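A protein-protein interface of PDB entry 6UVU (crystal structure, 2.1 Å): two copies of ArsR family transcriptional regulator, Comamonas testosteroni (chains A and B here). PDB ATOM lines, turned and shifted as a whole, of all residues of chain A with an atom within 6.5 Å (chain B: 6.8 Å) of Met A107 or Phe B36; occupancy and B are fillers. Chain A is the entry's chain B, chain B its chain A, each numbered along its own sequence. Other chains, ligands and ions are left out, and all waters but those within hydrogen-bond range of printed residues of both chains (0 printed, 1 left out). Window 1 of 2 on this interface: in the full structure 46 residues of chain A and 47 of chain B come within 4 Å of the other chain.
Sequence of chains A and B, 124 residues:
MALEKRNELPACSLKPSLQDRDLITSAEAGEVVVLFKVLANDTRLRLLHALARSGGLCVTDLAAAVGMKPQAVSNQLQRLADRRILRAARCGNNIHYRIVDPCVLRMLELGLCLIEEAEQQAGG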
ATOM      1  N   VAL A  32      -7.371  -5.470 -20.551  1.00  0.00           N
ATOM      2  CA  VAL A  32      -8.617  -5.469 -19.797  1.00  0.00           C
ATOM      3  C   VAL A  32      -9.608  -6.462 -20.399  1.00  0.00           C
ATOM      4  O   VAL A  32     -10.413  -7.064 -19.676  1.00  0.00           O
ATOM      5  CB  VAL A  32      -9.173  -4.031 -19.721  1.00  0.00           C
ATOM      6  CG1 VAL A  32     -10.675  -4.016 -19.842  1.00  0.00           C
ATOM      7  CG2 VAL A  32      -8.737  -3.363 -18.406  1.00  0.00           C
ATOM      8  N   LEU A  35      -9.188  -9.700 -18.764  1.00  0.00           N
ATOM      9  CA  LEU A  35      -9.901  -9.727 -17.485  1.00  0.00           C
ATOM     10  C   LEU A  35     -11.358 -10.149 -17.678  1.00  0.00           C
ATOM     11  O   LEU A  35     -11.840 -11.076 -17.015  1.00  0.00           O
ATOM     12  CB  LEU A  35      -9.804  -8.356 -16.809  1.00  0.00           C
ATOM     13  CG  LEU A  35     -10.715  -8.039 -15.614  1.00  0.00           C
ATOM     14  CD1 LEU A  35     -10.487  -9.019 -14.469  1.00  0.00           C
ATOM     15  CD2 LEU A  35     -10.491  -6.618 -15.149  1.00  0.00           C
ATOM     16  N   PHE A  36     -12.066  -9.507 -18.623  1.00  0.00           N
ATOM     17  CA  PHE A  36     -13.477  -9.815 -18.821  1.00  0.00           C
ATOM     18  C   PHE A  36     -13.688 -11.230 -19.362  1.00  0.00           C
ATOM     19  O   PHE A  36     -14.679 -11.886 -19.009  1.00  0.00           O
ATOM     20  CB  PHE A  36     -14.108  -8.783 -19.755  1.00  0.00           C
ATOM     21  CG  PHE A  36     -14.325  -7.437 -19.120  1.00  0.00           C
ATOM     22  CD1 PHE A  36     -15.225  -7.290 -18.081  1.00  0.00           C
ATOM     23  CD2 PHE A  36     -13.645  -6.314 -19.580  1.00  0.00           C
ATOM     24  CE1 PHE A  36     -15.441  -6.056 -17.506  1.00  0.00           C
ATOM     25  CE2 PHE A  36     -13.856  -5.062 -19.001  1.00  0.00           C
ATOM     26  CZ  PHE A  36     -14.758  -4.935 -17.964  1.00  0.00           C
ATOM     27  N   LYS A  37     -12.791 -11.713 -20.252  1.00  0.00           N
ATOM     28  CA  LYS A  37     -12.912 -13.084 -20.752  1.00  0.00           C
ATOM     29  C   LYS A  37     -12.845 -14.098 -19.612  1.00  0.00           C
ATOM     30  O   LYS A  37     -13.637 -15.046 -19.565  1.00  0.00           O
ATOM     31  CB  LYS A  37     -11.828 -13.391 -21.793  1.00  0.00           C
ATOM     32  CG  LYS A  37     -12.055 -12.784 -23.178  1.00  0.00           C
ATOM     33  CD  LYS A  37     -10.969 -13.228 -24.162  1.00  0.00           C
ATOM     34  CE  LYS A  37     -10.999 -12.399 -25.456  1.00  0.00           C
ATOM     35  NZ  LYS A  37      -9.844 -12.755 -26.339  1.00  0.00           N
ATOM     36  N   LEU A  39     -13.674 -13.609 -16.488  1.00  0.00           N
ATOM     37  CA  LEU A  39     -14.904 -13.529 -15.713  1.00  0.00           C
ATOM     38  C   LEU A  39     -16.163 -13.887 -16.501  1.00  0.00           C
ATOM     39  O   LEU A  39     -17.206 -14.142 -15.880  1.00  0.00           O
ATOM     40  CB  LEU A  39     -15.052 -12.123 -15.147  1.00  0.00           C
ATOM     41  CG  LEU A  39     -14.025 -11.811 -14.069  1.00  0.00           C
ATOM     42  CD1 LEU A  39     -13.928 -10.332 -13.955  1.00  0.00           C
ATOM     43  CD2 LEU A  39     -14.441 -12.458 -12.741  1.00  0.00           C
ATOM     44  N   ALA A  40     -16.105 -13.914 -17.837  1.00  0.00           N
ATOM     45  CA  ALA A  40     -17.318 -14.097 -18.636  1.00  0.00           C
ATOM     46  C   ALA A  40     -17.715 -15.561 -18.772  1.00  0.00           C
ATOM     47  O   ALA A  40     -17.901 -16.048 -19.899  1.00  0.00           O
ATOM     48  CB  ALA A  40     -17.134 -13.486 -20.031  1.00  0.00           C
ATOM     49  N   ASN A  41     -17.846 -16.263 -17.644  1.00  0.00           N
ATOM     50  CA  ASN A  41     -18.312 -17.644 -17.615  1.00  0.00           C
ATOM     51  C   ASN A  41     -19.009 -17.919 -16.287  1.00  0.00           C
ATOM     52  O   ASN A  41     -18.447 -17.671 -15.218  1.00  0.00           O
ATOM     53  CB  ASN A  41     -17.162 -18.633 -17.813  1.00  0.00           C
ATOM     54  CG  ASN A  41     -17.606 -20.082 -17.711  1.00  0.00           C
ATOM     55  OD1 ASN A  41     -17.565 -20.680 -16.638  1.00  0.00           O
ATOM     56  ND2 ASN A  41     -18.022 -20.655 -18.833  1.00  0.00           N
ATOM     57  N   LEU A  45     -17.204 -17.819 -12.535  1.00  0.00           N
ATOM     58  CA  LEU A  45     -17.549 -16.697 -11.676  1.00  0.00           C
ATOM     59  C   LEU A  45     -18.036 -17.190 -10.321  1.00  0.00           C
ATOM     60  O   LEU A  45     -17.696 -16.618  -9.283  1.00  0.00           O
ATOM     61  CB  LEU A  45     -18.613 -15.831 -12.364  1.00  0.00           C
ATOM     62  CG  LEU A  45     -18.945 -14.493 -11.697  1.00  0.00           C
ATOM     63  CD1 LEU A  45     -17.744 -13.555 -11.761  1.00  0.00           C
ATOM     64  CD2 LEU A  45     -20.176 -13.803 -12.310  1.00  0.00           C
ATOM     65  N   PRO A 102      -5.745  -9.114  -7.998  1.00  0.00           N
ATOM     66  CA  PRO A 102      -6.665  -8.123  -7.411  1.00  0.00           C
ATOM     67  C   PRO A 102      -7.589  -7.474  -8.438  1.00  0.00           C
ATOM     68  O   PRO A 102      -8.693  -7.049  -8.081  1.00  0.00           O
ATOM     69  CB  PRO A 102      -5.718  -7.094  -6.779  1.00  0.00           C
ATOM     70  CG  PRO A 102      -4.521  -7.133  -7.675  1.00  0.00           C
ATOM     71  CD  PRO A 102      -4.378  -8.582  -8.127  1.00  0.00           C
ATOM     72  N   CYS A 103      -7.174  -7.370  -9.700  1.00  0.00           N
ATOM     73  CA  CYS A 103      -8.079  -6.859 -10.722  1.00  0.00           C
ATOM     74  C   CYS A 103      -9.296  -7.753 -10.875  1.00  0.00           C
ATOM     75  O   CYS A 103     -10.426  -7.261 -10.973  1.00  0.00           O
ATOM     76  CB  CYS A 103      -7.344  -6.729 -12.054  1.00  0.00           C
ATOM     77  SG  CYS A 103      -5.996  -5.559 -11.976  1.00  0.00           S
ATOM     78  N   VAL A 104      -9.085  -9.067 -10.934  1.00  0.00           N
ATOM     79  CA  VAL A 104     -10.199 -10.008 -10.952  1.00  0.00           C
ATOM     80  C   VAL A 104     -11.080  -9.786  -9.734  1.00  0.00           C
ATOM     81  O   VAL A 104     -12.312  -9.812  -9.830  1.00  0.00           O
ATOM     82  CB  VAL A 104      -9.675 -11.456 -11.032  1.00  0.00           C
ATOM     83  CG1 VAL A 104     -10.663 -12.464 -10.404  1.00  0.00           C
ATOM     84  CG2 VAL A 104      -9.399 -11.835 -12.462  1.00  0.00           C
ATOM     85  N   LEU A 105     -10.458  -9.495  -8.583  1.00  0.00           N
ATOM     86  CA  LEU A 105     -11.208  -9.380  -7.338  1.00  0.00           C
ATOM     87  C   LEU A 105     -12.104  -8.147  -7.334  1.00  0.00           C
ATOM     88  O   LEU A 105     -13.276  -8.233  -6.971  1.00  0.00           O
ATOM     89  CB  LEU A 105     -10.256  -9.349  -6.148  1.00  0.00           C
ATOM     90  CG  LEU A 105     -10.976  -9.418  -4.810  1.00  0.00           C
ATOM     91  CD1 LEU A 105     -11.738 -10.736  -4.695  1.00  0.00           C
ATOM     92  CD2 LEU A 105      -9.961  -9.281  -3.686  1.00  0.00           C
ATOM     93  N   ARG A 106     -11.569  -6.987  -7.713  1.00  0.00           N
ATOM     94  CA  ARG A 106     -12.413  -5.794  -7.762  1.00  0.00           C
ATOM     95  C   ARG A 106     -13.553  -5.948  -8.766  1.00  0.00           C
ATOM     96  O   ARG A 106     -14.667  -5.446  -8.531  1.00  0.00           O
ATOM     97  CB  ARG A 106     -11.590  -4.557  -8.124  1.00  0.00           C
ATOM     98  CG  ARG A 106     -10.168  -4.528  -7.625  1.00  0.00           C
ATOM     99  CD  ARG A 106      -9.815  -3.175  -7.062  1.00  0.00           C
ATOM    100  NE  ARG A 106     -10.058  -2.066  -7.988  1.00  0.00           N
ATOM    101  CZ  ARG A 106      -9.099  -1.277  -8.477  1.00  0.00           C
ATOM    102  NH1 ARG A 106      -7.828  -1.477  -8.135  1.00  0.00           N
ATOM    103  NH2 ARG A 106      -9.399  -0.284  -9.312  1.00  0.00           N
ATOM    104  N   MET A 107     -13.303  -6.634  -9.882  1.00  0.00           N
ATOM    105  CA  MET A 107     -14.337  -6.795 -10.904  1.00  0.00           C
ATOM    106  C   MET A 107     -15.419  -7.758 -10.439  1.00  0.00           C
ATOM    107  O   MET A 107     -16.612  -7.520 -10.674  1.00  0.00           O
ATOM    108  CB  MET A 107     -13.714  -7.259 -12.227  1.00  0.00           C
ATOM    109  CG  MET A 107     -14.638  -7.086 -13.464  1.00  0.00           C
ATOM    110  SD  MET A 107     -15.241  -5.397 -13.812  1.00  0.00           S
ATOM    111  CE  MET A 107     -13.762  -4.657 -14.511  1.00  0.00           C
ATOM    112  N   LEU A 108     -15.025  -8.843  -9.762  1.00  0.00           N
ATOM    113  CA  LEU A 108     -16.002  -9.700  -9.096  1.00  0.00           C
ATOM    114  C   LEU A 108     -16.802  -8.925  -8.054  1.00  0.00           C
ATOM    115  O   LEU A 108     -18.024  -9.052  -7.996  1.00  0.00           O
ATOM    116  CB  LEU A 108     -15.304 -10.907  -8.453  1.00  0.00           C
ATOM    117  CG  LEU A 108     -16.017 -11.673  -7.334  1.00  0.00           C
ATOM    118  CD1 LEU A 108     -17.185 -12.476  -7.862  1.00  0.00           C
ATOM    119  CD2 LEU A 108     -15.043 -12.611  -6.571  1.00  0.00           C
ATOM    120  N   GLU A 109     -16.138  -8.106  -7.231  1.00  0.00           N
ATOM    121  CA  GLU A 109     -16.849  -7.338  -6.210  1.00  0.00           C
ATOM    122  C   GLU A 109     -17.850  -6.376  -6.837  1.00  0.00           C
ATOM    123  O   GLU A 109     -18.953  -6.182  -6.309  1.00  0.00           O
ATOM    124  CB  GLU A 109     -15.862  -6.564  -5.330  1.00  0.00           C
ATOM    125  CG  GLU A 109     -15.021  -7.426  -4.375  1.00  0.00           C
ATOM    126  CD  GLU A 109     -14.024  -6.578  -3.591  1.00  0.00           C
ATOM    127  OE1 GLU A 109     -14.017  -5.335  -3.788  1.00  0.00           O
ATOM    128  OE2 GLU A 109     -13.260  -7.140  -2.772  1.00  0.00           O
ATOM    129  N   LEU A 110     -17.474  -5.737  -7.947  1.00  0.00           N
ATOM    130  CA  LEU A 110     -18.413  -4.856  -8.641  1.00  0.00           C
ATOM    131  C   LEU A 110     -19.620  -5.640  -9.127  1.00  0.00           C
ATOM    132  O   LEU A 110     -20.770  -5.227  -8.930  1.00  0.00           O
ATOM    133  CB  LEU A 110     -17.731  -4.150  -9.812  1.00  0.00           C
ATOM    134  CG  LEU A 110     -18.679  -3.257 -10.631  1.00  0.00           C
ATOM    135  CD1 LEU A 110     -19.302  -2.170  -9.747  1.00  0.00           C
ATOM    136  CD2 LEU A 110     -17.944  -2.645 -11.823  1.00  0.00           C
ATOM    137  N   GLY A 111     -19.375  -6.792  -9.738  1.00  0.00           N
ATOM    138  CA  GLY A 111     -20.466  -7.672 -10.098  1.00  0.00           C
ATOM    139  C   GLY A 111     -21.375  -7.989  -8.928  1.00  0.00           C
ATOM    140  O   GLY A 111     -22.597  -8.008  -9.074  1.00  0.00           O
ATOM    141  N   LEU A 112     -20.789  -8.244  -7.749  1.00  0.00           N
ATOM    142  CA  LEU A 112     -21.594  -8.578  -6.576  1.00  0.00           C
ATOM    143  C   LEU A 112     -22.452  -7.394  -6.146  1.00  0.00           C
ATOM    144  O   LEU A 112     -23.626  -7.567  -5.801  1.00  0.00           O
ATOM    145  CB  LEU A 112     -20.692  -9.057  -5.420  1.00  0.00           C
ATOM    146  CG  LEU A 112     -19.885 -10.343  -5.679  1.00  0.00           C
ATOM    147  CD1 LEU A 112     -18.840 -10.602  -4.574  1.00  0.00           C
ATOM    148  CD2 LEU A 112     -20.789 -11.563  -5.846  1.00  0.00           C
ATOM    149  N   ALA B  29     -25.361 -15.394 -11.780  1.00  0.00           N
ATOM    150  CA  ALA B  29     -24.083 -15.365 -12.479  1.00  0.00           C
ATOM    151  C   ALA B  29     -24.268 -15.113 -13.970  1.00  0.00           C
ATOM    152  O   ALA B  29     -23.551 -14.292 -14.553  1.00  0.00           O
ATOM    153  CB  ALA B  29     -23.332 -16.679 -12.240  1.00  0.00           C
ATOM    154  N   GLU B  31     -26.579 -13.500 -15.585  1.00  0.00           N
ATOM    155  CA  GLU B  31     -26.939 -12.118 -15.891  1.00  0.00           C
ATOM    156  C   GLU B  31     -25.712 -11.215 -15.909  1.00  0.00           C
ATOM    157  O   GLU B  31     -25.552 -10.381 -16.806  1.00  0.00           O
ATOM    158  CB  GLU B  31     -27.965 -11.602 -14.878  1.00  0.00           C
ATOM    159  CG  GLU B  31     -29.312 -12.303 -14.936  1.00  0.00           C
ATOM    160  CD  GLU B  31     -30.310 -11.703 -13.955  1.00  0.00           C
ATOM    161  OE1 GLU B  31     -30.790 -10.569 -14.204  1.00  0.00           O
ATOM    162  OE2 GLU B  31     -30.608 -12.364 -12.929  1.00  0.00           O
ATOM    163  N   VAL B  32     -24.848 -11.339 -14.903  1.00  0.00           N
ATOM    164  CA  VAL B  32     -23.635 -10.528 -14.876  1.00  0.00           C
ATOM    165  C   VAL B  32     -22.676 -10.980 -15.980  1.00  0.00           C
ATOM    166  O   VAL B  32     -21.945 -10.165 -16.561  1.00  0.00           O
ATOM    167  CB  VAL B  32     -23.021 -10.603 -13.459  1.00  0.00           C
ATOM    168  CG1 VAL B  32     -21.531 -10.565 -13.492  1.00  0.00           C
ATOM    169  CG2 VAL B  32     -23.559  -9.467 -12.590  1.00  0.00           C
ATOM    170  N   VAL B  33     -22.702 -12.267 -16.322  1.00  0.00           N
ATOM    171  CA  VAL B  33     -21.795 -12.777 -17.340  1.00  0.00           C
ATOM    172  C   VAL B  33     -22.155 -12.214 -18.717  1.00  0.00           C
ATOM    173  O   VAL B  33     -21.265 -11.929 -19.530  1.00  0.00           O
ATOM    174  CB  VAL B  33     -21.794 -14.317 -17.312  1.00  0.00           C
ATOM    175  CG1 VAL B  33     -21.342 -14.888 -18.653  1.00  0.00           C
ATOM    176  CG2 VAL B  33     -20.879 -14.814 -16.172  1.00  0.00           C
ATOM    177  N   VAL B  34     -23.455 -12.014 -18.985  1.00  0.00           N
ATOM    178  CA  VAL B  34     -23.883 -11.308 -20.197  1.00  0.00           C
ATOM    179  C   VAL B  34     -23.140  -9.983 -20.340  1.00  0.00           C
ATOM    180  O   VAL B  34     -22.652  -9.628 -21.423  1.00  0.00           O
ATOM    181  CB  VAL B  34     -25.408 -11.078 -20.191  1.00  0.00           C
ATOM    182  CG1 VAL B  34     -25.819 -10.246 -21.420  1.00  0.00           C
ATOM    183  CG2 VAL B  34     -26.180 -12.407 -20.160  1.00  0.00           C
ATOM    184  N   LEU B  35     -23.049  -9.231 -19.248  1.00  0.00           N
ATOM    185  CA  LEU B  35     -22.368  -7.940 -19.275  1.00  0.00           C
ATOM    186  C   LEU B  35     -20.862  -8.106 -19.456  1.00  0.00           C
ATOM    187  O   LEU B  35     -20.242  -7.367 -20.231  1.00  0.00           O
ATOM    188  CB  LEU B  35     -22.685  -7.157 -17.998  1.00  0.00           C
ATOM    189  CG  LEU B  35     -24.180  -6.956 -17.702  1.00  0.00           C
ATOM    190  CD1 LEU B  35     -24.388  -5.984 -16.559  1.00  0.00           C
ATOM    191  CD2 LEU B  35     -24.927  -6.478 -18.953  1.00  0.00           C
ATOM    192  N   PHE B  36     -20.249  -9.065 -18.738  1.00  0.00           N
ATOM    193  CA  PHE B  36     -18.823  -9.327 -18.943  1.00  0.00           C
ATOM    194  C   PHE B  36     -18.540  -9.740 -20.390  1.00  0.00           C
ATOM    195  O   PHE B  36     -17.536  -9.317 -20.976  1.00  0.00           O
ATOM    196  CB  PHE B  36     -18.304 -10.412 -17.973  1.00  0.00           C
ATOM    197  CG  PHE B  36     -18.241  -9.983 -16.499  1.00  0.00           C
ATOM    198  CD1 PHE B  36     -18.026  -8.665 -16.136  1.00  0.00           C
ATOM    199  CD2 PHE B  36     -18.403 -10.920 -15.481  1.00  0.00           C
ATOM    200  CE1 PHE B  36     -17.974  -8.283 -14.799  1.00  0.00           C
ATOM    201  CE2 PHE B  36     -18.343 -10.539 -14.129  1.00  0.00           C
ATOM    202  CZ  PHE B  36     -18.142  -9.221 -13.790  1.00  0.00           C
ATOM    203  N   LYS B  37     -19.404 -10.581 -20.978  1.00  0.00           N
ATOM    204  CA  LYS B  37     -19.217 -10.972 -22.372  1.00  0.00           C
ATOM    205  C   LYS B  37     -19.248  -9.761 -23.292  1.00  0.00           C
ATOM    206  O   LYS B  37     -18.472  -9.673 -24.250  1.00  0.00           O
ATOM    207  CB  LYS B  37     -20.297 -11.960 -22.809  1.00  0.00           C
ATOM    208  CG  LYS B  37     -20.097 -13.405 -22.409  1.00  0.00           C
ATOM    209  CD  LYS B  37     -21.219 -14.259 -22.994  1.00  0.00           C
ATOM    210  CE  LYS B  37     -21.245 -15.638 -22.371  1.00  0.00           C
ATOM    211  NZ  LYS B  37     -19.949 -16.319 -22.573  1.00  0.00           N
ATOM    212  N   VAL B  38     -20.166  -8.827 -23.032  1.00  0.00           N
ATOM    213  CA  VAL B  38     -20.256  -7.634 -23.863  1.00  0.00           C
ATOM    214  C   VAL B  38     -18.940  -6.874 -23.849  1.00  0.00           C
ATOM    215  O   VAL B  38     -18.451  -6.449 -24.902  1.00  0.00           O
ATOM    216  CB  VAL B  38     -21.436  -6.764 -23.407  1.00  0.00           C
ATOM    217  CG1 VAL B  38     -21.276  -5.331 -23.922  1.00  0.00           C
ATOM    218  CG2 VAL B  38     -22.733  -7.381 -23.900  1.00  0.00           C
ATOM    219  N   LEU B  39     -18.311  -6.736 -22.677  1.00  0.00           N
ATOM    220  CA  LEU B  39     -17.076  -5.967 -22.598  1.00  0.00           C
ATOM    221  C   LEU B  39     -15.823  -6.748 -22.992  1.00  0.00           C
ATOM    222  O   LEU B  39     -14.766  -6.125 -23.148  1.00  0.00           O
ATOM    223  CB  LEU B  39     -16.887  -5.419 -21.184  1.00  0.00           C
ATOM    224  CG  LEU B  39     -17.921  -4.402 -20.699  1.00  0.00           C
ATOM    225  CD1 LEU B  39     -18.145  -4.693 -19.244  1.00  0.00           C
ATOM    226  CD2 LEU B  39     -17.416  -2.991 -20.858  1.00  0.00           C
ATOM    227  N   ALA B  40     -15.899  -8.077 -23.131  1.00  0.00           N
ATOM    228  CA  ALA B  40     -14.736  -8.903 -23.479  1.00  0.00           C
ATOM    229  C   ALA B  40     -14.502  -8.940 -24.996  1.00  0.00           C
ATOM    230  O   ALA B  40     -14.466 -10.001 -25.625  1.00  0.00           O
ATOM    231  CB  ALA B  40     -14.908 -10.310 -22.915  1.00  0.00           C
ATOM    232  N   ASN B  41     -14.300  -7.749 -25.568  1.00  0.00           N
ATOM    233  CA  ASN B  41     -14.101  -7.571 -27.004  1.00  0.00           C
ATOM    234  C   ASN B  41     -13.555  -6.166 -27.240  1.00  0.00           C
ATOM    235  O   ASN B  41     -14.164  -5.185 -26.787  1.00  0.00           O
ATOM    236  CB  ASN B  41     -15.429  -7.766 -27.758  1.00  0.00           C
ATOM    237  CG  ASN B  41     -15.297  -7.541 -29.259  1.00  0.00           C
ATOM    238  OD1 ASN B  41     -15.174  -6.405 -29.732  1.00  0.00           O
ATOM    239  ND2 ASN B  41     -15.357  -8.626 -30.015  1.00  0.00           N
ATOM    240  N   ARG B  44     -15.954  -3.636 -29.092  1.00  0.00           N
ATOM    241  CA  ARG B  44     -17.074  -3.199 -28.255  1.00  0.00           C
ATOM    242  C   ARG B  44     -16.604  -2.259 -27.152  1.00  0.00           C
ATOM    243  O   ARG B  44     -17.231  -1.225 -26.912  1.00  0.00           O
ATOM    244  CB  ARG B  44     -17.838  -4.398 -27.673  1.00  0.00           C
ATOM    245  CG  ARG B  44     -18.719  -5.068 -28.749  1.00  0.00           C
ATOM    246  CD  ARG B  44     -19.736  -6.049 -28.149  1.00  0.00           C
ATOM    247  NE  ARG B  44     -19.121  -7.166 -27.458  1.00  0.00           N
ATOM    248  CZ  ARG B  44     -18.847  -8.339 -28.031  1.00  0.00           C
ATOM    249  NH1 ARG B  44     -19.110  -8.524 -29.317  1.00  0.00           N
ATOM    250  NH2 ARG B  44     -18.298  -9.324 -27.322  1.00  0.00           N
ATOM    251  N   ARG B 106     -20.559   1.302 -15.339  1.00  0.00           N
ATOM    252  CA  ARG B 106     -19.716   1.130 -14.159  1.00  0.00           C
ATOM    253  C   ARG B 106     -18.605   0.107 -14.404  1.00  0.00           C
ATOM    254  O   ARG B 106     -17.466   0.295 -13.963  1.00  0.00           O
ATOM    255  CB  ARG B 106     -20.588   0.733 -12.971  1.00  0.00           C
ATOM    256  CG  ARG B 106     -21.480   1.865 -12.504  1.00  0.00           C
ATOM    257  CD  ARG B 106     -22.579   1.348 -11.612  1.00  0.00           C
ATOM    258  NE  ARG B 106     -22.080   0.596 -10.449  1.00  0.00           N
ATOM    259  CZ  ARG B 106     -22.804   0.373  -9.352  1.00  0.00           C
ATOM    260  NH1 ARG B 106     -24.034   0.856  -9.280  1.00  0.00           N
ATOM    261  NH2 ARG B 106     -22.307  -0.323  -8.328  1.00  0.00           N
ATOM    262  N   MET B 107     -18.908  -0.976 -15.110  1.00  0.00           N
ATOM    263  CA  MET B 107     -17.849  -1.936 -15.449  1.00  0.00           C
ATOM    264  C   MET B 107     -16.758  -1.296 -16.309  1.00  0.00           C
ATOM    265  O   MET B 107     -15.558  -1.501 -16.069  1.00  0.00           O
ATOM    266  CB  MET B 107     -18.450  -3.131 -16.166  1.00  0.00           C
ATOM    267  CG  MET B 107     -19.265  -4.038 -15.282  1.00  0.00           C
ATOM    268  SD  MET B 107     -19.895  -5.399 -16.272  1.00  0.00           S
ATOM    269  CE  MET B 107     -20.754  -6.371 -15.036  1.00  0.00           C
ATOM    270  N   LEU B 108     -17.161  -0.511 -17.309  1.00  0.00           N
ATOM    271  CA  LEU B 108     -16.214   0.212 -18.155  1.00  0.00           C
ATOM    272  C   LEU B 108     -15.368   1.172 -17.338  1.00  0.00           C
ATOM    273  O   LEU B 108     -14.150   1.258 -17.530  1.00  0.00           O
ATOM    274  CB  LEU B 108     -16.972   0.978 -19.242  1.00  0.00           C
ATOM    275  CG  LEU B 108     -16.186   1.896 -20.188  1.00  0.00           C
ATOM    276  CD1 LEU B 108     -15.266   1.068 -21.108  1.00  0.00           C
ATOM    277  CD2 LEU B 108     -17.121   2.803 -21.037  1.00  0.00           C
ATOM    278  N   LEU B 110     -14.559   1.016 -14.162  1.00  0.00           N
ATOM    279  CA  LEU B 110     -13.569   0.262 -13.403  1.00  0.00           C
ATOM    280  C   LEU B 110     -12.432  -0.199 -14.311  1.00  0.00           C
ATOM    281  O   LEU B 110     -11.254  -0.125 -13.932  1.00  0.00           O
ATOM    282  CB  LEU B 110     -14.236  -0.923 -12.701  1.00  0.00           C
ATOM    283  CG  LEU B 110     -13.276  -1.884 -11.978  1.00  0.00           C
ATOM    284  CD1 LEU B 110     -12.480  -1.129 -10.925  1.00  0.00           C
ATOM    285  CD2 LEU B 110     -14.019  -3.045 -11.344  1.00  0.00           C
ATOM    286  N   GLY B 111     -12.761  -0.636 -15.533  1.00  0.00           N
ATOM    287  CA  GLY B 111     -11.723  -0.973 -16.506  1.00  0.00           C
ATOM    288  C   GLY B 111     -10.813   0.198 -16.832  1.00  0.00           C
ATOM    289  O   GLY B 111      -9.603   0.029 -16.996  1.00  0.00           O
ATOM    290  N   LEU B 114      -8.403   0.675 -13.943  1.00  0.00           N
ATOM    291  CA  LEU B 114      -7.312  -0.293 -13.973  1.00  0.00           C
ATOM    292  C   LEU B 114      -6.241   0.092 -14.986  1.00  0.00           C
ATOM    293  O   LEU B 114      -5.058  -0.184 -14.766  1.00  0.00           O
ATOM    294  CB  LEU B 114      -7.862  -1.688 -14.276  1.00  0.00           C
ATOM    295  CG  LEU B 114      -8.848  -2.205 -13.225  1.00  0.00           C
ATOM    296  CD1 LEU B 114      -9.405  -3.551 -13.624  1.00  0.00           C
ATOM    297  CD2 LEU B 114      -8.183  -2.289 -11.853  1.00  0.00           C
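O of Ala A40 sits at hydrogen-bond distance from NZ of Lys B37 (3.4 Å).
Of the printed residues of chain B, Ala A40 touches Val B33, Phe B36 and Lys B37.
Pro A102 touches none of the printed residues of chain B.
Met A107 touches just these residues of chain B: Phe B36 (3.8 Å), Met B107 (3.95 Å) and Leu B110 (3.6 Å).
Of the printed residues of chain A, Val B32 touches Leu A45 (3.7 Å) and Gly A111 (3.9 Å).
Of chain A, only Phe A36 (3.7 Å), Leu A39 (3.5 Å), Ala A40 (3.9 Å), Leu A45 (3.9 Å) and Met A107 (3.8 Å) come within 4 Å of Phe B36.
Asn B41 touches none of the printed residues of chain A.
Of the printed residues of chain A, Leu B114 touches Leu A35, Cys A103 and Arg A106.
The nearest residue of chain B that does not touch Met A107 is Gly B111 (4.3 Å).
The nearest residue of chain A that does not touch Phe B36 is Gly A111 (4.6 Å).
The nearest printed residue of chain B that does not touch Arg A106 is Gly B111 (7.1 Å).
The backbone carbonyl oxygen (O) of Lys B37 lies within hydrogen-bond range of the guanidinium group (NH2) of Arg B44, at 3.1 Å.
Phe B36 touches Phe A36 (CD1 to CD1, 3.7 Å).
CB of Phe A36 touches CB of Ala B40 (3.6 Å).
Leu A39 touches Val B33.
CD2 of Phe B36 touches O of Leu A39 (3.5 Å).
CG1 of Val B33 touches C of Ala A40, at 3.7 Å.
CG1 of Val B32 touches CD2 of Leu A45, 3.7 Å away.
Leu A45 touches Phe B36 (CD1 to CE2, 3.9 Å).
Met A107 touches Phe B36 (CG to CE1, 3.8 Å).
Leu A110 touches Arg B106 (CD2 to O, 3.7 Å).
Leu A110 touches Met B107.
Of the 19 printed residues of chain B, 11 touch a printed residue of chain A.
Hydrophobic or aromatic side chains of chain B within 4 Å of the printed part of chain A: Val B32, Val B33, Phe B36, Leu B39, Ala B40, Met B107, Leu B110 and Leu B114.
Among the printed residues, 24 pairs touch across the chains.
Among the printed residues, no Asp or Glu carboxylate lies within 4 Å of a Lys or Arg side-chain nitrogen of the other chain.
Phe A36 touches Ala B40, and with the chains exchanged Ala A40 touches Phe B36.
Lys A37 touches Ala B40, and with the chains exchanged Ala A40 touches Lys B37.
Arg A106 touches Leu B110, and with the chains exchanged Leu A110 touches Arg B106.
Leu B110 touches its own counterpart, Leu A110.
Positions printed for both chains: 32, 35, 36, 37, 39, 40, 41, 106, 107, 108, 110 and 111.
Of the 24 pairs that touch across the chains among the printed residues, 15 have their exchanged pair printed and touching as well.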
